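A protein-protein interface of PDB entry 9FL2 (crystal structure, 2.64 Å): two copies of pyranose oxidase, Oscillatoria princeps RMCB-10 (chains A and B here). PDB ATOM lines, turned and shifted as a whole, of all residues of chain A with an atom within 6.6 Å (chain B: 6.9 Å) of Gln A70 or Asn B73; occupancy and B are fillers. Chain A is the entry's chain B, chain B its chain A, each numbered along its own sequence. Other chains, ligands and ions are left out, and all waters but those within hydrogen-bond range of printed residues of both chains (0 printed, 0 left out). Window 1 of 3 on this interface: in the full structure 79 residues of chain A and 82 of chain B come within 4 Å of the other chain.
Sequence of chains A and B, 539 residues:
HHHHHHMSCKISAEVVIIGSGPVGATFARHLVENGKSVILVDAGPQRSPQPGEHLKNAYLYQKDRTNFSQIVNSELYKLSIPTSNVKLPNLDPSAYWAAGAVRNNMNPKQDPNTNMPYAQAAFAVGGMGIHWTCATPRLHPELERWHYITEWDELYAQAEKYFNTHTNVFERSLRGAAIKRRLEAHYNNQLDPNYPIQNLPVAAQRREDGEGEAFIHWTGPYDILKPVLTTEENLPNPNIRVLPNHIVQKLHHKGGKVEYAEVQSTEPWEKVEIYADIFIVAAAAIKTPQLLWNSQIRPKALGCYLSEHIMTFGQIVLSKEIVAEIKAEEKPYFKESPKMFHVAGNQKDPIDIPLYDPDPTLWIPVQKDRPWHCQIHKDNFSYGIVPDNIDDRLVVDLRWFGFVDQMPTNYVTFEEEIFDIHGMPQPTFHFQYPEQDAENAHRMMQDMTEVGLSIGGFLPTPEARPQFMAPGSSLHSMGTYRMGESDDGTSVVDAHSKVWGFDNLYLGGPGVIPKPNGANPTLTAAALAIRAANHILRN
The backbone carbonyl oxygen (O) of Ile B71 lies within hydrogen-bond range of the side-chain hydroxyl (OG) of Ser B74 (2.7 Å).
The backbone carbonyl oxygen (O) of Ile A71 lies within hydrogen-bond range of the side-chain hydroxyl (OG) of Ser A74 (2.7 Å).
Asn A67 touches Tyr B77 (ND2 to CD1, 3.5 Å).
Gln A70 touches Gln B70.
Gln A70 touches Asn B73 (OE1 to CB, 3.3 Å).
O of Gln A70 touches CB of Ser B74 (3.5 Å).
Ser B74 touches Ile A71.
Asn A73 touches Gln B70 (CB to OE1, 3.2 Å).
O of Gln B70 touches CB of Ser A74 (3.5 Å).
Ile B71 touches Ser A74 (CD1 to OG, 3.6 Å).
Asn B73 touches one residue of chain A.
Of the printed residues of chain B, Ser A74 touches Gln B70 (3.5 Å) and Ile B71 (3.6 Å).
Of the printed residues of chain A, Ile B71 touches Ser A74 (3.6 Å).
Printed residues of chain A within 4 Å of Ser B74: Gln A70 and Ile A71.
Printed residues of chain B within 4 Å of Ile A71: Ser B74.
Phe B381 touches none of the printed residues of chain A.
The nearest residue of chain A that does not touch Asn B73 is Asn A67 (5.5 Å).
The nearest printed residue of chain A that does not touch Ile B71 is Glu A75 (5.6 Å).
Hydrophobic or aromatic side chains of chain A within 4 Å of the printed part of chain B: Ile A71.
Of the 15 printed residues of chain B, 5 touch a printed residue of chain A.
Printed residues of chain B that touch a printed residue of chain A: Gln B70, Ile B71, Asn B73, Ser B74 and Tyr B77.
Hydrophobic or aromatic side chains of chain B that line the printed part of chain A: Ile B71 and Tyr B77.
Among the printed residues, no Asp or Glu carboxylate lies within 4 Å of a Lys or Arg side-chain nitrogen of the other chain.
Gln B70 touches its own counterpart, Gln A70.
Gln A70 touches Asn B73, and with the chains exchanged Asn A73 touches Gln B70.
Gln A70 touches Ser B74, and with the chains exchanged Ser A74 touches Gln B70.
Ile A71 touches Ser B74, and with the chains exchanged Ser A74 touches Ile B71.
10 positions are printed for both chains.
Of the 8 pairs that touch across the chains among the printed residues, 7 have their exchanged pair printed and touching as well.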
ATOM      1  N   TYR A  61      -0.147  -2.788  -0.076  1.00  0.00           N
ATOM      2  CA  TYR A  61       0.068  -2.052  -1.314  1.00  0.00           C
ATOM      3  C   TYR A  61       0.845  -0.781  -1.020  1.00  0.00           C
ATOM      4  O   TYR A  61       1.582  -0.269  -1.868  1.00  0.00           O
ATOM      5  CB  TYR A  61      -1.276  -1.803  -2.006  1.00  0.00           C
ATOM      6  CG  TYR A  61      -1.899  -3.133  -2.388  1.00  0.00           C
ATOM      7  CD1 TYR A  61      -1.184  -4.067  -3.130  1.00  0.00           C
ATOM      8  CD2 TYR A  61      -3.151  -3.508  -1.924  1.00  0.00           C
ATOM      9  CE1 TYR A  61      -1.725  -5.304  -3.449  1.00  0.00           C
ATOM     10  CE2 TYR A  61      -3.704  -4.746  -2.232  1.00  0.00           C
ATOM     11  CZ  TYR A  61      -2.982  -5.648  -2.989  1.00  0.00           C
ATOM     12  OH  TYR A  61      -3.512  -6.869  -3.279  1.00  0.00           O
ATOM     13  N   THR A  66       4.401  -2.437  -6.652  1.00  0.00           N
ATOM     14  CA  THR A  66       4.433  -3.286  -7.842  1.00  0.00           C
ATOM     15  C   THR A  66       3.379  -4.389  -7.779  1.00  0.00           C
ATOM     16  O   THR A  66       2.881  -4.839  -8.818  1.00  0.00           O
ATOM     17  CB  THR A  66       5.834  -3.884  -7.995  1.00  0.00           C
ATOM     18  OG1 THR A  66       6.639  -2.752  -8.286  1.00  0.00           O
ATOM     19  CG2 THR A  66       6.000  -4.820  -9.166  1.00  0.00           C
ATOM     20  N   ASN A  67       3.040  -4.813  -6.556  1.00  0.00           N
ATOM     21  CA  ASN A  67       2.164  -5.951  -6.361  1.00  0.00           C
ATOM     22  C   ASN A  67       0.721  -5.659  -6.739  1.00  0.00           C
ATOM     23  O   ASN A  67      -0.027  -6.588  -7.041  1.00  0.00           O
ATOM     24  CB  ASN A  67       2.102  -6.392  -4.910  1.00  0.00           C
ATOM     25  CG  ASN A  67       1.388  -7.709  -4.797  1.00  0.00           C
ATOM     26  OD1 ASN A  67       0.197  -7.752  -4.474  1.00  0.00           O
ATOM     27  ND2 ASN A  67       2.090  -8.771  -5.136  1.00  0.00           N
ATOM     28  N   PHE A  68       0.331  -4.385  -6.673  1.00  0.00           N
ATOM     29  CA  PHE A  68      -1.050  -3.993  -6.920  1.00  0.00           C
ATOM     30  C   PHE A  68      -1.451  -4.232  -8.373  1.00  0.00           C
ATOM     31  O   PHE A  68      -2.638  -4.318  -8.660  1.00  0.00           O
ATOM     32  CB  PHE A  68      -1.309  -2.528  -6.560  1.00  0.00           C
ATOM     33  CG  PHE A  68      -2.788  -2.196  -6.496  1.00  0.00           C
ATOM     34  CD1 PHE A  68      -3.556  -2.632  -5.427  1.00  0.00           C
ATOM     35  CD2 PHE A  68      -3.407  -1.479  -7.496  1.00  0.00           C
ATOM     36  CE1 PHE A  68      -4.909  -2.342  -5.359  1.00  0.00           C
ATOM     37  CE2 PHE A  68      -4.758  -1.189  -7.421  1.00  0.00           C
ATOM     38  CZ  PHE A  68      -5.508  -1.625  -6.353  1.00  0.00           C
ATOM     39  N   SER A  69      -0.473  -4.351  -9.268  1.00  0.00           N
ATOM     40  CA  SER A  69      -0.746  -4.717 -10.644  1.00  0.00           C
ATOM     41  C   SER A  69      -1.532  -6.039 -10.722  1.00  0.00           C
ATOM     42  O   SER A  69      -2.250  -6.311 -11.685  1.00  0.00           O
ATOM     43  CB  SER A  69       0.537  -4.780 -11.423  1.00  0.00           C
ATOM     44  OG  SER A  69       1.175  -3.513 -11.461  1.00  0.00           O
ATOM     45  N   GLN A  70      -1.412  -6.881  -9.698  1.00  0.00           N
ATOM     46  CA  GLN A  70      -2.061  -8.180  -9.722  1.00  0.00           C
ATOM     47  C   GLN A  70      -3.545  -7.996  -9.443  1.00  0.00           C
ATOM     48  O   GLN A  70      -4.364  -8.788  -9.904  1.00  0.00           O
ATOM     49  CB  GLN A  70      -1.440  -9.099  -8.675  1.00  0.00           C
ATOM     50  CG  GLN A  70       0.053  -9.277  -8.874  1.00  0.00           C
ATOM     51  CD  GLN A  70       0.315 -10.018 -10.155  1.00  0.00           C
ATOM     52  OE1 GLN A  70       0.016 -11.212 -10.255  1.00  0.00           O
ATOM     53  NE2 GLN A  70       0.861  -9.313 -11.130  1.00  0.00           N
ATOM     54  N   ILE A  71      -3.880  -6.957  -8.673  1.00  0.00           N
ATOM     55  CA  ILE A  71      -5.277  -6.638  -8.464  1.00  0.00           C
ATOM     56  C   ILE A  71      -5.843  -6.093  -9.762  1.00  0.00           C
ATOM     57  O   ILE A  71      -6.975  -6.405 -10.127  1.00  0.00           O
ATOM     58  CB  ILE A  71      -5.446  -5.664  -7.293  1.00  0.00           C
ATOM     59  CG1 ILE A  71      -5.153  -6.373  -5.990  1.00  0.00           C
ATOM     60  CG2 ILE A  71      -6.840  -5.017  -7.276  1.00  0.00           C
ATOM     61  CD1 ILE A  71      -6.257  -7.311  -5.543  1.00  0.00           C
ATOM     62  N   VAL A  72      -5.041  -5.273 -10.446  1.00  0.00           N
ATOM     63  CA  VAL A  72      -5.472  -4.695 -11.707  1.00  0.00           C
ATOM     64  C   VAL A  72      -5.805  -5.833 -12.664  1.00  0.00           C
ATOM     65  O   VAL A  72      -6.897  -5.872 -13.214  1.00  0.00           O
ATOM     66  CB  VAL A  72      -4.443  -3.729 -12.332  1.00  0.00           C
ATOM     67  CG1 VAL A  72      -4.797  -3.368 -13.777  1.00  0.00           C
ATOM     68  CG2 VAL A  72      -4.246  -2.468 -11.491  1.00  0.00           C
ATOM     69  N   ASN A  73      -4.867  -6.772 -12.837  1.00  0.00           N
ATOM     70  CA  ASN A  73      -5.083  -7.846 -13.786  1.00  0.00           C
ATOM     71  C   ASN A  73      -6.364  -8.583 -13.440  1.00  0.00           C
ATOM     72  O   ASN A  73      -7.061  -9.000 -14.346  1.00  0.00           O
ATOM     73  CB  ASN A  73      -3.894  -8.783 -13.838  1.00  0.00           C
ATOM     74  CG  ASN A  73      -2.710  -8.094 -14.443  1.00  0.00           C
ATOM     75  OD1 ASN A  73      -2.838  -7.028 -15.070  1.00  0.00           O
ATOM     76  ND2 ASN A  73      -1.559  -8.707 -14.250  1.00  0.00           N
ATOM     77  N   SER A  74      -6.676  -8.669 -12.145  1.00  0.00           N
ATOM     78  CA  SER A  74      -7.874  -9.338 -11.676  1.00  0.00           C
ATOM     79  C   SER A  74      -9.124  -8.503 -11.942  1.00  0.00           C
ATOM     80  O   SER A  74     -10.226  -9.020 -11.868  1.00  0.00           O
ATOM     81  CB  SER A  74      -7.803  -9.662 -10.216  1.00  0.00           C
ATOM     82  OG  SER A  74      -8.323  -8.596  -9.430  1.00  0.00           O
ATOM     83  N   GLU A  75      -8.980  -7.214 -12.223  1.00  0.00           N
ATOM     84  CA  GLU A  75     -10.151  -6.371 -12.387  1.00  0.00           C
ATOM     85  C   GLU A  75     -10.527  -6.214 -13.866  1.00  0.00           C
ATOM     86  O   GLU A  75     -11.692  -5.988 -14.201  1.00  0.00           O
ATOM     87  CB  GLU A  75      -9.813  -5.042 -11.714  1.00  0.00           C
ATOM     88  CG  GLU A  75      -9.833  -5.125 -10.195  1.00  0.00           C
ATOM     89  CD  GLU A  75     -11.249  -5.210  -9.684  1.00  0.00           C
ATOM     90  OE1 GLU A  75     -12.102  -4.370 -10.085  1.00  0.00           O
ATOM     91  OE2 GLU A  75     -11.484  -6.127  -8.878  1.00  0.00           O
ATOM     92  N   ASN A 380       0.664   1.356 -11.007  1.00  0.00           N
ATOM     93  CA  ASN A 380       0.408  -0.062 -11.126  1.00  0.00           C
ATOM     94  C   ASN A 380      -0.612  -0.294 -12.233  1.00  0.00           C
ATOM     95  O   ASN A 380      -1.753   0.156 -12.141  1.00  0.00           O
ATOM     96  CB  ASN A 380      -0.068  -0.580  -9.782  1.00  0.00           C
ATOM     97  CG  ASN A 380       0.713   0.083  -8.677  1.00  0.00           C
ATOM     98  OD1 ASN A 380       0.207   0.994  -8.006  1.00  0.00           O
ATOM     99  ND2 ASN A 380       1.978  -0.284  -8.557  1.00  0.00           N
ATOM    100  N   PHE A 381      -0.149  -1.006 -13.263  1.00  0.00           N
ATOM    101  CA  PHE A 381      -0.906  -1.310 -14.464  1.00  0.00           C
ATOM    102  C   PHE A 381      -0.574  -2.739 -14.871  1.00  0.00           C
ATOM    103  O   PHE A 381       0.347  -3.336 -14.330  1.00  0.00           O
ATOM    104  CB  PHE A 381      -0.527  -0.401 -15.636  1.00  0.00           C
ATOM    105  CG  PHE A 381      -0.929   1.068 -15.547  1.00  0.00           C
ATOM    106  CD1 PHE A 381      -0.155   1.982 -14.822  1.00  0.00           C
ATOM    107  CD2 PHE A 381      -2.038   1.539 -16.255  1.00  0.00           C
ATOM    108  CE1 PHE A 381      -0.522   3.323 -14.779  1.00  0.00           C
ATOM    109  CE2 PHE A 381      -2.391   2.877 -16.199  1.00  0.00           C
ATOM    110  CZ  PHE A 381      -1.628   3.764 -15.467  1.00  0.00           C
ATOM    111  N   ILE A 385       5.326  -4.186 -15.200  1.00  0.00           N
ATOM    112  CA  ILE A 385       5.449  -4.473 -13.788  1.00  0.00           C
ATOM    113  C   ILE A 385       6.921  -4.719 -13.539  1.00  0.00           C
ATOM    114  O   ILE A 385       7.543  -5.461 -14.285  1.00  0.00           O
ATOM    115  CB  ILE A 385       4.589  -5.685 -13.399  1.00  0.00           C
ATOM    116  CG1 ILE A 385       3.117  -5.411 -13.695  1.00  0.00           C
ATOM    117  CG2 ILE A 385       4.811  -6.075 -11.941  1.00  0.00           C
ATOM    118  CD1 ILE A 385       2.224  -6.623 -13.543  1.00  0.00           C
ATOM    119  N   PHE B  68     -10.400 -16.624 -12.859  1.00  0.00           N
ATOM    120  CA  PHE B  68     -10.231 -16.553 -11.424  1.00  0.00           C
ATOM    121  C   PHE B  68      -8.766 -16.732 -11.019  1.00  0.00           C
ATOM    122  O   PHE B  68      -8.393 -16.348  -9.923  1.00  0.00           O
ATOM    123  CB  PHE B  68     -11.089 -17.605 -10.725  1.00  0.00           C
ATOM    124  CG  PHE B  68     -11.199 -17.344  -9.235  1.00  0.00           C
ATOM    125  CD1 PHE B  68     -12.004 -16.320  -8.763  1.00  0.00           C
ATOM    126  CD2 PHE B  68     -10.489 -18.093  -8.319  1.00  0.00           C
ATOM    127  CE1 PHE B  68     -12.107 -16.069  -7.413  1.00  0.00           C
ATOM    128  CE2 PHE B  68     -10.605 -17.835  -6.975  1.00  0.00           C
ATOM    129  CZ  PHE B  68     -11.407 -16.824  -6.524  1.00  0.00           C
ATOM    130  N   SER B  69      -7.944 -17.303 -11.894  1.00  0.00           N
ATOM    131  CA  SER B  69      -6.514 -17.376 -11.663  1.00  0.00           C
ATOM    132  C   SER B  69      -5.916 -15.983 -11.408  1.00  0.00           C
ATOM    133  O   SER B  69      -4.867 -15.834 -10.774  1.00  0.00           O
ATOM    134  CB  SER B  69      -5.835 -18.064 -12.818  1.00  0.00           C
ATOM    135  OG  SER B  69      -6.291 -19.397 -12.963  1.00  0.00           O
ATOM    136  N   GLN B  70      -6.577 -14.933 -11.894  1.00  0.00           N
ATOM    137  CA  GLN B  70      -6.055 -13.585 -11.732  1.00  0.00           C
ATOM    138  C   GLN B  70      -6.282 -13.121 -10.308  1.00  0.00           C
ATOM    139  O   GLN B  70      -5.510 -12.328  -9.796  1.00  0.00           O
ATOM    140  CB  GLN B  70      -6.734 -12.635 -12.720  1.00  0.00           C
ATOM    141  CG  GLN B  70      -6.520 -13.060 -14.166  1.00  0.00           C
ATOM    142  CD  GLN B  70      -5.059 -12.942 -14.520  1.00  0.00           C
ATOM    143  OE1 GLN B  70      -4.507 -11.836 -14.575  1.00  0.00           O
ATOM    144  NE2 GLN B  70      -4.419 -14.088 -14.702  1.00  0.00           N
ATOM    145  N   ILE B  71      -7.350 -13.620  -9.692  1.00  0.00           N
ATOM    146  CA  ILE B  71      -7.585 -13.337  -8.291  1.00  0.00           C
ATOM    147  C   ILE B  71      -6.528 -14.075  -7.481  1.00  0.00           C
ATOM    148  O   ILE B  71      -5.998 -13.530  -6.512  1.00  0.00           O
ATOM    149  CB  ILE B  71      -9.021 -13.726  -7.891  1.00  0.00           C
ATOM    150  CG1 ILE B  71     -10.003 -12.760  -8.502  1.00  0.00           C
ATOM    151  CG2 ILE B  71      -9.199 -13.798  -6.376  1.00  0.00           C
ATOM    152  CD1 ILE B  71      -9.984 -11.380  -7.862  1.00  0.00           C
ATOM    153  N   VAL B  72      -6.228 -15.314  -7.890  1.00  0.00           N
ATOM    154  CA  VAL B  72      -5.237 -16.107  -7.200  1.00  0.00           C
ATOM    155  C   VAL B  72      -3.919 -15.344  -7.224  1.00  0.00           C
ATOM    156  O   VAL B  72      -3.318 -15.121  -6.185  1.00  0.00           O
ATOM    157  CB  VAL B  72      -5.067 -17.526  -7.774  1.00  0.00           C
ATOM    158  CG1 VAL B  72      -3.817 -18.225  -7.219  1.00  0.00           C
ATOM    159  CG2 VAL B  72      -6.323 -18.387  -7.596  1.00  0.00           C
ATOM    160  N   ASN B  73      -3.472 -14.931  -8.408  1.00  0.00           N
ATOM    161  CA  ASN B  73      -2.186 -14.267  -8.508  1.00  0.00           C
ATOM    162  C   ASN B  73      -2.164 -13.042  -7.614  1.00  0.00           C
ATOM    163  O   ASN B  73      -1.128 -12.743  -7.045  1.00  0.00           O
ATOM    164  CB  ASN B  73      -1.841 -13.941  -9.943  1.00  0.00           C
ATOM    165  CG  ASN B  73      -1.563 -15.209 -10.704  1.00  0.00           C
ATOM    166  OD1 ASN B  73      -1.333 -16.278 -10.109  1.00  0.00           O
ATOM    167  ND2 ASN B  73      -1.592 -15.098 -12.021  1.00  0.00           N
ATOM    168  N   SER B  74      -3.324 -12.410  -7.442  1.00  0.00           N
ATOM    169  CA  SER B  74      -3.448 -11.234  -6.598  1.00  0.00           C
ATOM    170  C   SER B  74      -3.421 -11.606  -5.124  1.00  0.00           C
ATOM    171  O   SER B  74      -3.232 -10.746  -4.288  1.00  0.00           O
ATOM    172  CB  SER B  74      -4.704 -10.452  -6.895  1.00  0.00           C
ATOM    173  OG  SER B  74      -5.781 -10.906  -6.086  1.00  0.00           O
ATOM    174  N   GLU B  75      -3.634 -12.867  -4.785  1.00  0.00           N
ATOM    175  CA  GLU B  75      -3.709 -13.249  -3.385  1.00  0.00           C
ATOM    176  C   GLU B  75      -2.371 -13.788  -2.886  1.00  0.00           C
ATOM    177  O   GLU B  75      -2.095 -13.736  -1.696  1.00  0.00           O
ATOM    178  CB  GLU B  75      -4.840 -14.267  -3.273  1.00  0.00           C
ATOM    179  CG  GLU B  75      -6.211 -13.615  -3.381  1.00  0.00           C
ATOM    180  CD  GLU B  75      -6.542 -12.848  -2.123  1.00  0.00           C
ATOM    181  OE1 GLU B  75      -6.465 -13.457  -1.024  1.00  0.00           O
ATOM    182  OE2 GLU B  75      -6.885 -11.655  -2.260  1.00  0.00           O
ATOM    183  N   LEU B  76      -1.558 -14.322  -3.796  1.00  0.00           N
ATOM    184  CA  LEU B  76      -0.395 -15.099  -3.408  1.00  0.00           C
ATOM    185  C   LEU B  76       0.832 -14.217  -3.403  1.00  0.00           C
ATOM    186  O   LEU B  76       1.121 -13.607  -4.424  1.00  0.00           O
ATOM    187  CB  LEU B  76      -0.175 -16.261  -4.375  1.00  0.00           C
ATOM    188  CG  LEU B  76      -1.169 -17.419  -4.274  1.00  0.00           C
ATOM    189  CD1 LEU B  76      -0.656 -18.562  -5.138  1.00  0.00           C
ATOM    190  CD2 LEU B  76      -1.366 -17.855  -2.846  1.00  0.00           C
ATOM    191  N   TYR B  77       1.579 -14.248  -2.293  1.00  0.00           N
ATOM    192  CA  TYR B  77       2.726 -13.378  -2.134  1.00  0.00           C
ATOM    193  C   TYR B  77       3.935 -14.210  -1.722  1.00  0.00           C
ATOM    194  O   TYR B  77       3.909 -14.813  -0.657  1.00  0.00           O
ATOM    195  CB  TYR B  77       2.377 -12.289  -1.115  1.00  0.00           C
ATOM    196  CG  TYR B  77       3.310 -11.083  -1.173  1.00  0.00           C
ATOM    197  CD1 TYR B  77       3.088 -10.032  -2.064  1.00  0.00           C
ATOM    198  CD2 TYR B  77       4.443 -11.007  -0.370  1.00  0.00           C
ATOM    199  CE1 TYR B  77       3.943  -8.939  -2.131  1.00  0.00           C
ATOM    200  CE2 TYR B  77       5.299  -9.917  -0.427  1.00  0.00           C
ATOM    201  CZ  TYR B  77       5.045  -8.872  -1.299  1.00  0.00           C
ATOM    202  OH  TYR B  77       5.913  -7.822  -1.337  1.00  0.00           O
ATOM    203  N   GLN B 120       4.485 -19.264  -0.622  1.00  0.00           N
ATOM    204  CA  GLN B 120       3.758 -18.014  -0.619  1.00  0.00           C
ATOM    205  C   GLN B 120       2.744 -17.998   0.518  1.00  0.00           C
ATOM    206  O   GLN B 120       2.417 -19.034   1.074  1.00  0.00           O
ATOM    207  CB  GLN B 120       3.021 -17.884  -1.948  1.00  0.00           C
ATOM    208  CG  GLN B 120       3.928 -17.827  -3.171  1.00  0.00           C
ATOM    209  CD  GLN B 120       3.165 -18.068  -4.457  1.00  0.00           C
ATOM    210  OE1 GLN B 120       2.800 -17.125  -5.162  1.00  0.00           O
ATOM    211  NE2 GLN B 120       2.942 -19.329  -4.789  1.00  0.00           N
ATOM    212  N   PHE B 381      -5.423 -21.752 -10.739  1.00  0.00           N
ATOM    213  CA  PHE B 381      -4.152 -21.660 -10.046  1.00  0.00           C
ATOM    214  C   PHE B 381      -3.276 -20.668 -10.797  1.00  0.00           C
ATOM    215  O   PHE B 381      -3.616 -20.261 -11.900  1.00  0.00           O
ATOM    216  CB  PHE B 381      -3.415 -23.001  -9.996  1.00  0.00           C
ATOM    217  CG  PHE B 381      -4.011 -24.097  -9.122  1.00  0.00           C
ATOM    218  CD1 PHE B 381      -5.057 -24.892  -9.593  1.00  0.00           C
ATOM    219  CD2 PHE B 381      -3.479 -24.355  -7.859  1.00  0.00           C
ATOM    220  CE1 PHE B 381      -5.584 -25.893  -8.798  1.00  0.00           C
ATOM    221  CE2 PHE B 381      -4.004 -25.366  -7.075  1.00  0.00           C
ATOM    222  CZ  PHE B 381      -5.050 -26.136  -7.548  1.00  0.00           C
ATOM    223  N   SER B 382      -2.129 -20.334 -10.198  1.00  0.00           N
ATOM    224  CA  SER B 382      -1.140 -19.431 -10.776  1.00  0.00           C
ATOM    225  C   SER B 382      -0.637 -19.977 -12.110  1.00  0.00           C
ATOM    226  O   SER B 382      -0.277 -19.214 -12.992  1.00  0.00           O
ATOM    227  CB  SER B 382       0.037 -19.212  -9.841  1.00  0.00           C
ATOM    228  OG  SER B 382      -0.313 -19.251  -8.461  1.00  0.00           O
ATOM    229  N   TYR B 383      -0.596 -21.303 -12.245  1.00  0.00           N
ATOM    230  CA  TYR B 383       0.062 -21.942 -13.369  1.00  0.00           C
ATOM    231  C   TYR B 383      -1.001 -22.605 -14.231  1.00  0.00           C
ATOM    232  O   TYR B 383      -2.139 -22.782 -13.811  1.00  0.00           O
ATOM    233  CB  TYR B 383       1.100 -22.940 -12.849  1.00  0.00           C
ATOM    234  CG  TYR B 383       0.561 -23.913 -11.804  1.00  0.00           C
ATOM    235  CD1 TYR B 383       0.472 -23.559 -10.459  1.00  0.00           C
ATOM    236  CD2 TYR B 383       0.151 -25.192 -12.160  1.00  0.00           C
ATOM    237  CE1 TYR B 383      -0.041 -24.430  -9.509  1.00  0.00           C
ATOM    238  CE2 TYR B 383      -0.331 -26.086 -11.217  1.00  0.00           C
ATOM    239  CZ  TYR B 383      -0.456 -25.694  -9.892  1.00  0.00           C
ATOM    240  OH  TYR B 383      -0.952 -26.530  -8.932  1.00  0.00           O
ATOM    241  N   ILE B 385      -2.862 -21.638 -16.675  1.00  0.00           N
ATOM    242  CA  ILE B 385      -4.072 -20.929 -17.023  1.00  0.00           C
ATOM    243  C   ILE B 385      -4.281 -21.187 -18.498  1.00  0.00           C
ATOM    244  O   ILE B 385      -3.334 -21.059 -19.276  1.00  0.00           O
ATOM    245  CB  ILE B 385      -3.915 -19.427 -16.733  1.00  0.00           C
ATOM    246  CG1 ILE B 385      -3.616 -19.210 -15.252  1.00  0.00           C
ATOM    247  CG2 ILE B 385      -5.136 -18.642 -17.215  1.00  0.00           C
ATOM    248  CD1 ILE B 385      -3.302 -17.789 -14.873  1.00  0.00           C
